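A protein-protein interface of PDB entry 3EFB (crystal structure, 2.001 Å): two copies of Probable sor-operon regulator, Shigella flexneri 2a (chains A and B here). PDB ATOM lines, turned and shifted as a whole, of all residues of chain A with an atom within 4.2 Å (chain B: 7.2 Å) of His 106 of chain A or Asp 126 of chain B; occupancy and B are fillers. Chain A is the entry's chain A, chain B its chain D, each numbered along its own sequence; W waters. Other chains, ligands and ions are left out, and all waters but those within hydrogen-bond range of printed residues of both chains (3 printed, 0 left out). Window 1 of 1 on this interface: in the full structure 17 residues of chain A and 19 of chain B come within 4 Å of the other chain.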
ATOM      1  N   GLY A  96     -14.180 -26.624  12.967  1.00  0.00           N
ATOM      2  CA  GLY A  96     -15.027 -25.452  13.031  1.00  0.00           C
ATOM      3  C   GLY A  96     -15.990 -25.494  14.193  1.00  0.00           C
ATOM      4  O   GLY A  96     -16.308 -26.570  14.693  1.00  0.00           O
ATOM      5  N   PRO A  97     -16.482 -24.316  14.615  1.00  0.00           N
ATOM      6  CA  PRO A  97     -17.377 -24.173  15.772  1.00  0.00           C
ATOM      7  C   PRO A  97     -18.844 -24.500  15.494  1.00  0.00           C
ATOM      8  O   PRO A  97     -19.665 -24.370  16.407  1.00  0.00           O
ATOM      9  CB  PRO A  97     -17.264 -22.686  16.127  1.00  0.00           C
ATOM     10  CG  PRO A  97     -16.767 -21.999  14.880  1.00  0.00           C
ATOM     11  CD  PRO A  97     -16.275 -23.045  13.907  1.00  0.00           C
ATOM     12  N   SER A  98     -19.173 -24.908  14.275  1.00  0.00           N
ATOM     13  CA  SER A  98     -20.563 -25.162  13.916  1.00  0.00           C
ATOM     14  C   SER A  98     -21.520 -24.021  14.322  1.00  0.00           C
ATOM     15  O   SER A  98     -22.559 -24.256  14.952  1.00  0.00           O
ATOM     16  CB  SER A  98     -21.020 -26.500  14.509  1.00  0.00           C
ATOM     17  OG  SER A  98     -20.387 -27.579  13.836  1.00  0.00           O
ATOM     18  N   GLU A 102     -19.126 -16.333  16.147  1.00  0.00           N
ATOM     19  CA  GLU A 102     -19.186 -15.458  14.974  1.00  0.00           C
ATOM     20  C   GLU A 102     -18.062 -15.819  14.012  1.00  0.00           C
ATOM     21  O   GLU A 102     -16.976 -16.200  14.434  1.00  0.00           O
ATOM     22  CB  GLU A 102     -18.936 -13.999  15.351  1.00  0.00           C
ATOM     23  CG  GLU A 102     -19.569 -13.503  16.623  1.00  0.00           C
ATOM     24  CD  GLU A 102     -19.233 -12.046  16.861  1.00  0.00           C
ATOM     25  OE1 GLU A 102     -19.092 -11.304  15.865  1.00  0.00           O
ATOM     26  OE2 GLU A 102     -19.098 -11.638  18.032  1.00  0.00           O
ATOM     27  N   SER A 103     -18.313 -15.628  12.724  1.00  0.00           N
ATOM     28  CA  SER A 103     -17.350 -15.942  11.678  1.00  0.00           C
ATOM     29  C   SER A 103     -16.001 -15.298  11.927  1.00  0.00           C
ATOM     30  O   SER A 103     -14.970 -15.852  11.582  1.00  0.00           O
ATOM     31  CB  SER A 103     -17.901 -15.481  10.321  1.00  0.00           C
ATOM     32  OG  SER A 103     -19.185 -16.055  10.104  1.00  0.00           O
ATOM     33  N   ARG A 104     -16.032 -14.110  12.514  1.00  0.00           N
ATOM     34  CA  ARG A 104     -14.831 -13.349  12.830  1.00  0.00           C
ATOM     35  C   ARG A 104     -13.812 -14.196  13.593  1.00  0.00           C
ATOM     36  O   ARG A 104     -12.603 -14.029  13.427  1.00  0.00           O
ATOM     37  CB  ARG A 104     -15.211 -12.143  13.695  1.00  0.00           C
ATOM     38  CG  ARG A 104     -14.328 -10.930  13.510  1.00  0.00           C
ATOM     39  CD  ARG A 104     -14.512  -9.932  14.650  1.00  0.00           C
ATOM     40  NE  ARG A 104     -15.816 -10.042  15.301  1.00  0.00           N
ATOM     41  CZ  ARG A 104     -16.291  -9.150  16.169  1.00  0.00           C
ATOM     42  NH1 ARG A 104     -17.482  -9.319  16.726  1.00  0.00           N
ATOM     43  NH2 ARG A 104     -15.572  -8.079  16.477  1.00  0.00           N
ATOM     44  N   TYR A 105     -14.312 -15.090  14.438  1.00  0.00           N
ATOM     45  CA  TYR A 105     -13.463 -15.843  15.376  1.00  0.00           C
ATOM     46  C   TYR A 105     -13.342 -17.308  15.032  1.00  0.00           C
ATOM     47  O   TYR A 105     -12.769 -18.108  15.804  1.00  0.00           O
ATOM     48  CB  TYR A 105     -13.989 -15.715  16.809  1.00  0.00           C
ATOM     49  CG  TYR A 105     -14.170 -14.284  17.253  1.00  0.00           C
ATOM     50  CD1 TYR A 105     -13.141 -13.360  17.098  1.00  0.00           C
ATOM     51  CD2 TYR A 105     -15.369 -13.856  17.816  1.00  0.00           C
ATOM     52  CE1 TYR A 105     -13.287 -12.059  17.508  1.00  0.00           C
ATOM     53  CE2 TYR A 105     -15.538 -12.541  18.219  1.00  0.00           C
ATOM     54  CZ  TYR A 105     -14.486 -11.649  18.067  1.00  0.00           C
ATOM     55  OH  TYR A 105     -14.633 -10.336  18.458  1.00  0.00           O
ATOM     56  N   HIS A 106     -13.864 -17.655  13.864  1.00  0.00           N
ATOM     57  CA  HIS A 106     -13.742 -18.996  13.339  1.00  0.00           C
ATOM     58  C   HIS A 106     -12.256 -19.353  13.173  1.00  0.00           C
ATOM     59  O   HIS A 106     -11.457 -18.537  12.710  1.00  0.00           O
ATOM     60  CB  HIS A 106     -14.476 -19.041  12.007  1.00  0.00           C
ATOM     61  CG  HIS A 106     -14.768 -20.418  11.500  1.00  0.00           C
ATOM     62  ND1 HIS A 106     -13.782 -21.335  11.207  1.00  0.00           N
ATOM     63  CD2 HIS A 106     -15.940 -20.997  11.130  1.00  0.00           C
ATOM     64  CE1 HIS A 106     -14.334 -22.441  10.739  1.00  0.00           C
ATOM     65  NE2 HIS A 106     -15.644 -22.256  10.668  1.00  0.00           N
ATOM     66  N   VAL A 107     -11.887 -20.571  13.567  1.00  0.00           N
ATOM     67  CA  VAL A 107     -10.496 -21.018  13.438  1.00  0.00           C
ATOM     68  C   VAL A 107      -9.984 -20.879  11.995  1.00  0.00           C
ATOM     69  O   VAL A 107      -8.846 -20.466  11.793  1.00  0.00           O
ATOM     70  CB  VAL A 107     -10.283 -22.458  13.985  1.00  0.00           C
ATOM     71  CG1 VAL A 107     -10.950 -23.495  13.064  1.00  0.00           C
ATOM     72  CG2 VAL A 107      -8.752 -22.769  14.189  1.00  0.00           C
ATOM     73  N   ASN A 108     -10.813 -21.176  10.985  1.00  0.00           N
ATOM     74  CA  ASN A 108     -10.357 -21.027   9.597  1.00  0.00           C
ATOM     75  C   ASN A 108     -10.111 -19.562   9.213  1.00  0.00           C
ATOM     76  O   ASN A 108      -9.185 -19.220   8.428  1.00  0.00           O
ATOM     77  CB  ASN A 108     -11.352 -21.709   8.609  1.00  0.00           C
ATOM     78  CG  ASN A 108     -11.166 -23.225   8.546  1.00  0.00           C
ATOM     79  OD1 ASN A 108     -10.103 -23.733   8.905  1.00  0.00           O
ATOM     80  ND2 ASN A 108     -12.188 -23.952   8.104  1.00  0.00           N
ATOM     81  N   THR A 109     -10.948 -18.684   9.749  1.00  0.00           N
ATOM     82  CA  THR A 109     -10.821 -17.256   9.493  1.00  0.00           C
ATOM     83  C   THR A 109      -9.470 -16.788  10.026  1.00  0.00           C
ATOM     84  O   THR A 109      -8.740 -16.044   9.352  1.00  0.00           O
ATOM     85  CB  THR A 109     -11.933 -16.417  10.203  1.00  0.00           C
ATOM     86  OG1 THR A 109     -13.248 -16.825   9.768  1.00  0.00           O
ATOM     87  CG2 THR A 109     -11.744 -14.945   9.920  1.00  0.00           C
ATOM     88  N   LEU A 110      -9.146 -17.227  11.241  1.00  0.00           N
ATOM     89  CA  LEU A 110      -7.919 -16.801  11.914  1.00  0.00           C
ATOM     90  C   LEU A 110      -6.687 -17.347  11.224  1.00  0.00           C
ATOM     91  O   LEU A 110      -5.702 -16.643  11.050  1.00  0.00           O
ATOM     92  CB  LEU A 110      -7.922 -17.273  13.381  1.00  0.00           C
ATOM     93  CG  LEU A 110      -9.078 -16.684  14.187  1.00  0.00           C
ATOM     94  CD1 LEU A 110      -8.961 -17.024  15.692  1.00  0.00           C
ATOM     95  CD2 LEU A 110      -9.162 -15.166  13.900  1.00  0.00           C
ATOM     96  N   PHE A 127     -14.071 -29.675   8.612  1.00  0.00           N
ATOM     97  CA  PHE A 127     -14.826 -30.551   9.480  1.00  0.00           C
ATOM     98  C   PHE A 127     -15.085 -29.759  10.735  1.00  0.00           C
ATOM     99  O   PHE A 127     -14.345 -28.801  11.030  1.00  0.00           O
ATOM    100  CB  PHE A 127     -14.060 -31.847   9.790  1.00  0.00           C
ATOM    101  CG  PHE A 127     -12.657 -31.622  10.214  1.00  0.00           C
ATOM    102  CD1 PHE A 127     -11.623 -31.668   9.286  1.00  0.00           C
ATOM    103  CD2 PHE A 127     -12.358 -31.373  11.544  1.00  0.00           C
ATOM    104  CE1 PHE A 127     -10.304 -31.449   9.679  1.00  0.00           C
ATOM    105  CE2 PHE A 127     -11.039 -31.158  11.940  1.00  0.00           C
ATOM    106  CZ  PHE A 127     -10.015 -31.191  11.000  1.00  0.00           C
ATOM    107  N   PRO A 128     -16.151 -30.127  11.465  1.00  0.00           N
ATOM    108  CA  PRO A 128     -16.541 -29.474  12.718  1.00  0.00           C
ATOM    109  C   PRO A 128     -15.712 -29.983  13.892  1.00  0.00           C
ATOM    110  O   PRO A 128     -15.204 -31.101  13.848  1.00  0.00           O
ATOM    111  CB  PRO A 128     -18.002 -29.919  12.914  1.00  0.00           C
ATOM    112  CG  PRO A 128     -18.355 -30.782  11.719  1.00  0.00           C
ATOM    113  CD  PRO A 128     -17.072 -31.225  11.111  1.00  0.00           C
ATOM    114  N   PRO B  92     -22.509 -19.982   2.366  1.00  0.00           N
ATOM    115  CA  PRO B  92     -21.970 -20.817   1.295  1.00  0.00           C
ATOM    116  C   PRO B  92     -23.084 -21.734   0.817  1.00  0.00           C
ATOM    117  O   PRO B  92     -23.901 -22.131   1.654  1.00  0.00           O
ATOM    118  CB  PRO B  92     -20.921 -21.679   2.010  1.00  0.00           C
ATOM    119  CG  PRO B  92     -20.955 -21.285   3.426  1.00  0.00           C
ATOM    120  CD  PRO B  92     -22.190 -20.530   3.692  1.00  0.00           C
ATOM    121  N   GLY B  95     -20.305 -27.183   0.546  1.00  0.00           N
ATOM    122  CA  GLY B  95     -19.344 -27.399   1.617  1.00  0.00           C
ATOM    123  C   GLY B  95     -17.927 -27.053   1.169  1.00  0.00           C
ATOM    124  O   GLY B  95     -17.708 -26.693   0.013  1.00  0.00           O
ATOM    125  N   GLY B  96     -16.961 -27.166   2.077  1.00  0.00           N
ATOM    126  CA  GLY B  96     -15.563 -26.878   1.763  1.00  0.00           C
ATOM    127  C   GLY B  96     -14.912 -27.846   0.778  1.00  0.00           C
ATOM    128  O   GLY B  96     -15.344 -28.989   0.655  1.00  0.00           O
ATOM    129  N   ASN B 108     -15.914 -20.685   2.095  1.00  0.00           N
ATOM    130  CA  ASN B 108     -15.987 -19.861   3.300  1.00  0.00           C
ATOM    131  C   ASN B 108     -15.187 -18.563   3.213  1.00  0.00           C
ATOM    132  O   ASN B 108     -15.627 -17.523   3.705  1.00  0.00           O
ATOM    133  CB  ASN B 108     -15.556 -20.655   4.541  1.00  0.00           C
ATOM    134  CG  ASN B 108     -16.600 -21.647   4.977  1.00  0.00           C
ATOM    135  OD1 ASN B 108     -17.785 -21.461   4.727  1.00  0.00           O
ATOM    136  ND2 ASN B 108     -16.163 -22.731   5.582  1.00  0.00           N
ATOM    137  N   TYR B 112     -17.174 -15.081   3.580  1.00  0.00           N
ATOM    138  CA  TYR B 112     -16.735 -14.157   4.619  1.00  0.00           C
ATOM    139  C   TYR B 112     -16.347 -12.809   4.047  1.00  0.00           C
ATOM    140  O   TYR B 112     -16.740 -11.771   4.586  1.00  0.00           O
ATOM    141  CB  TYR B 112     -15.550 -14.762   5.414  1.00  0.00           C
ATOM    142  CG  TYR B 112     -15.102 -13.902   6.573  1.00  0.00           C
ATOM    143  CD1 TYR B 112     -15.851 -13.840   7.732  1.00  0.00           C
ATOM    144  CD2 TYR B 112     -13.924 -13.154   6.509  1.00  0.00           C
ATOM    145  CE1 TYR B 112     -15.447 -13.064   8.800  1.00  0.00           C
ATOM    146  CE2 TYR B 112     -13.509 -12.369   7.579  1.00  0.00           C
ATOM    147  CZ  TYR B 112     -14.296 -12.325   8.720  1.00  0.00           C
ATOM    148  OH  TYR B 112     -13.939 -11.569   9.802  1.00  0.00           O
ATOM    149  N   HIS B 123     -22.609 -16.953   7.592  1.00  0.00           N
ATOM    150  CA  HIS B 123     -22.659 -18.191   8.341  1.00  0.00           C
ATOM    151  C   HIS B 123     -21.886 -19.209   7.528  1.00  0.00           C
ATOM    152  O   HIS B 123     -22.323 -19.577   6.443  1.00  0.00           O
ATOM    153  CB  HIS B 123     -24.109 -18.626   8.570  1.00  0.00           C
ATOM    154  CG  HIS B 123     -24.918 -17.595   9.287  1.00  0.00           C
ATOM    155  ND1 HIS B 123     -24.821 -17.386  10.642  1.00  0.00           N
ATOM    156  CD2 HIS B 123     -25.791 -16.666   8.828  1.00  0.00           C
ATOM    157  CE1 HIS B 123     -25.628 -16.403  10.999  1.00  0.00           C
ATOM    158  NE2 HIS B 123     -26.231 -15.949   9.916  1.00  0.00           N
ATOM    159  N   LEU B 124     -20.734 -19.635   8.064  1.00  0.00           N
ATOM    160  CA  LEU B 124     -19.771 -20.476   7.343  1.00  0.00           C
ATOM    161  C   LEU B 124     -20.109 -21.945   7.514  1.00  0.00           C
ATOM    162  O   LEU B 124     -20.637 -22.327   8.550  1.00  0.00           O
ATOM    163  CB  LEU B 124     -18.336 -20.208   7.849  1.00  0.00           C
ATOM    164  CG  LEU B 124     -17.939 -18.737   7.846  1.00  0.00           C
ATOM    165  CD1 LEU B 124     -16.431 -18.568   8.087  1.00  0.00           C
ATOM    166  CD2 LEU B 124     -18.338 -18.114   6.513  1.00  0.00           C
ATOM    167  N   ALA B 125     -19.812 -22.760   6.502  1.00  0.00           N
ATOM    168  CA  ALA B 125     -20.086 -24.185   6.579  1.00  0.00           C
ATOM    169  C   ALA B 125     -18.875 -24.961   7.082  1.00  0.00           C
ATOM    170  O   ALA B 125     -17.760 -24.810   6.574  1.00  0.00           O
ATOM    171  CB  ALA B 125     -20.545 -24.726   5.243  1.00  0.00           C
ATOM    172  N   ASP B 126     -19.102 -25.778   8.103  1.00  0.00           N
ATOM    173  CA  ASP B 126     -18.050 -26.606   8.665  1.00  0.00           C
ATOM    174  C   ASP B 126     -18.303 -28.061   8.327  1.00  0.00           C
ATOM    175  O   ASP B 126     -18.151 -28.936   9.172  1.00  0.00           O
ATOM    176  CB  ASP B 126     -18.005 -26.458  10.184  1.00  0.00           C
ATOM    177  CG  ASP B 126     -17.654 -25.058  10.612  1.00  0.00           C
ATOM    178  OD1 ASP B 126     -17.022 -24.337   9.814  1.00  0.00           O
ATOM    179  OD2 ASP B 126     -18.017 -24.684  11.745  1.00  0.00           O
ATOM    180  N   PHE B 127     -18.707 -28.315   7.093  1.00  0.00           N
ATOM    181  CA  PHE B 127     -18.795 -29.680   6.581  1.00  0.00           C
ATOM    182  C   PHE B 127     -18.167 -29.670   5.202  1.00  0.00           C
ATOM    183  O   PHE B 127     -18.096 -28.619   4.569  1.00  0.00           O
ATOM    184  CB  PHE B 127     -20.246 -30.155   6.508  1.00  0.00           C
ATOM    185  CG  PHE B 127     -21.183 -29.153   5.892  1.00  0.00           C
ATOM    186  CD1 PHE B 127     -21.921 -28.292   6.689  1.00  0.00           C
ATOM    187  CD2 PHE B 127     -21.337 -29.080   4.514  1.00  0.00           C
ATOM    188  CE1 PHE B 127     -22.814 -27.371   6.114  1.00  0.00           C
ATOM    189  CE2 PHE B 127     -22.230 -28.171   3.939  1.00  0.00           C
ATOM    190  CZ  PHE B 127     -22.967 -27.320   4.738  1.00  0.00           C
ATOM    191  N   PRO B 128     -17.684 -30.834   4.739  1.00  0.00           N
ATOM    192  CA  PRO B 128     -17.061 -30.874   3.416  1.00  0.00           C
ATOM    193  C   PRO B 128     -18.125 -30.949   2.325  1.00  0.00           C
ATOM    194  O   PRO B 128     -19.212 -31.444   2.561  1.00  0.00           O
ATOM    195  CB  PRO B 128     -16.275 -32.187   3.423  1.00  0.00           C
ATOM    196  CG  PRO B 128     -16.669 -32.915   4.685  1.00  0.00           C
ATOM    197  CD  PRO B 128     -17.765 -32.166   5.358  1.00  0.00           C
ATOM    198  N   ILE B 140     -24.079 -36.283   8.661  1.00  0.00           N
ATOM    199  CA  ILE B 140     -23.788 -34.865   8.820  1.00  0.00           C
ATOM    200  C   ILE B 140     -25.006 -34.052   8.405  1.00  0.00           C
ATOM    201  O   ILE B 140     -25.299 -32.991   8.959  1.00  0.00           O
ATOM    202  CB  ILE B 140     -22.563 -34.435   7.991  1.00  0.00           C
ATOM    203  CG1 ILE B 140     -21.270 -34.842   8.707  1.00  0.00           C
ATOM    204  CG2 ILE B 140     -22.594 -32.935   7.752  1.00  0.00           C
ATOM    205  CD1 ILE B 140     -20.098 -34.973   7.788  1.00  0.00           C
ATOM    206  N   HIS B 145     -26.204 -27.950  12.794  1.00  0.00           N
ATOM    207  CA  HIS B 145     -25.429 -27.045  11.930  1.00  0.00           C
ATOM    208  C   HIS B 145     -25.772 -27.162  10.430  1.00  0.00           C
ATOM    209  O   HIS B 145     -26.072 -26.161   9.785  1.00  0.00           O
ATOM    210  CB  HIS B 145     -23.909 -27.216  12.179  1.00  0.00           C
ATOM    211  CG  HIS B 145     -23.045 -26.432  11.239  1.00  0.00           C
ATOM    212  ND1 HIS B 145     -23.053 -25.054  11.190  1.00  0.00           N
ATOM    213  CD2 HIS B 145     -22.126 -26.832  10.329  1.00  0.00           C
ATOM    214  CE1 HIS B 145     -22.191 -24.640  10.282  1.00  0.00           C
ATOM    215  NE2 HIS B 145     -21.612 -25.700   9.747  1.00  0.00           N
ATOM    216  N   ILE B 149     -27.691 -24.353   7.955  1.00  0.00           N
ATOM    217  CA  ILE B 149     -27.197 -23.845   6.665  1.00  0.00           C
ATOM    218  C   ILE B 149     -28.219 -24.184   5.575  1.00  0.00           C
ATOM    219  O   ILE B 149     -28.556 -23.367   4.725  1.00  0.00           O
ATOM    220  CB  ILE B 149     -25.823 -24.476   6.299  1.00  0.00           C
ATOM    221  CG1 ILE B 149     -24.772 -24.151   7.362  1.00  0.00           C
ATOM    222  CG2 ILE B 149     -25.333 -23.968   4.948  1.00  0.00           C
ATOM    223  CD1 ILE B 149     -24.456 -22.657   7.425  1.00  0.00           C
HETATM  224  O   HOH W   1     -14.893 -24.840   7.071  1.00  0.00           O
HETATM  225  O   HOH W   2     -20.167 -18.284  10.852  1.00  0.00           O
HETATM  226  O   HOH W   3     -14.788 -25.984   9.686  1.00  0.00           O
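Of chain B, only Leu 124 (3.9 Å) and Asp 126 (2.6 Å) come within 4 Å of His 106 of chain A.
Of the printed residues of chain A, Asp 126 of chain B touches Gly 96 (3.3 Å), Pro 97 (3.2 Å), Ser 98 (2.8 Å), His 106 (2.6 Å), Phe 127 (3.5 Å) and Pro 128 (3.2 Å).
Of the printed residues of chain B, Arg 104 of chain A touches Tyr 112 (3.6 Å).
Of the printed residues of chain B, Ser 103 of chain A touches Tyr 112 (3.7 Å) and Leu 124 (3.7 Å).
Of the printed residues of chain A, Tyr 112 of chain B touches Ser 103 (3.7 Å), Arg 104 (3.6 Å) and Thr 109 (3.8 Å).
Ala 125 of chain B touches none of the printed residues of chain A.
Glu 102 of chain A touches none of the printed residues of chain B.
The nearest residue of chain B that does not touch His 106 of chain A is Asn 108 of chain B (5.1 Å).
Positions printed for both chains: 96, 108, 127 and 128.
Water W2 lies within hydrogen-bond range of the side-chain hydroxyl of Ser 103 of chain A (2.5 Å) and the backbone NH of Leu 124 of chain B (3.1 Å).
Water W3 lies within hydrogen-bond range of OD1 of Asp 126 of chain B (2.8 Å), O of Phe 127 of chain A (3.2 Å) and N of Gly 96 of chain A (3.4 Å).
Water W1 lies within hydrogen-bond range of the side-chain amide nitrogen (ND2) of Asn 108 of chain B (2.9 Å), the backbone carbonyl oxygen (O) of Ala 125 of chain B (2.9 Å) and the side-chain amide nitrogen (ND2) of Asn 108 of chain A (3.0 Å).
Hydrophobic or aromatic side chains of chain B within 4 Å of the printed part of chain A: Tyr 112, Leu 124 and His 145.
Along chain B the printed residues that touch a printed residue of chain A span positions 112 to 145.
Of the 14 printed residues of chain A, 9 touch a printed residue of chain B.
Hydrophobic or aromatic side chains of chain A within 4 Å of the printed part of chain B: Pro 97, His 106 and Pro 128.
ND1 of His 106 of chain A sits at hydrogen-bond distance from N of Asn 108 of chain A.
The backbone carbonyl oxygen (O) of Ser 103 of chain A lies within hydrogen-bond range of the side-chain hydroxyl (OG1) of Thr 109 of chain A, at 2.7 Å.
NH2 of Arg 104 of chain A lies close to OH of Tyr 105 of chain A (3.1 Å).
The backbone carbonyl oxygen (O) of Phe 127 of chain A sits at hydrogen-bond distance from the backbone NH (N) of Gly 96 of chain A (2.9 Å).
The side-chain carboxylate (OE1) of Glu 102 of chain A is in salt-bridge range of the guanidinium group (NH1) of Arg 104 of chain A (2.7 Å).
NE2 of His 145 of chain B lies within hydrogen-bond range of N of Asp 126 of chain B.
Among the printed residues, pairs that only touch across the chains: Gly 96 of chain A with Asp 126 of chain B, Phe 127 of chain A with Asp 126 of chain B, Arg 104 of chain A with Tyr 112 of chain B, Ser 98 of chain A with His 145 of chain B, Ser 103 of chain A with Tyr 112 of chain B, Ser 103 of chain A with Leu 124 of chain B, Thr 109 of chain A with Tyr 112 of chain B, His 106 of chain A with Leu 124 of chain B and Thr 109 of chain A with Leu 124 of chain B.
A ring nitrogen (NE2) of His 106 of chain A lies within hydrogen-bond range of the side-chain carboxylate (OD1) of Asp 126 of chain B (2.6 Å).
OD2 of Asp 126 of chain B sits close to N of Pro 97 of chain A (3.3 Å).
The backbone nitrogen of Pro 128 of chain A sits close to the backbone carbonyl oxygen of Asp 126 of chain B (3.3 Å).
N of Ser 98 of chain A is in hydrogen-bond range of OD2 of Asp 126 of chain B (2.8 Å).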
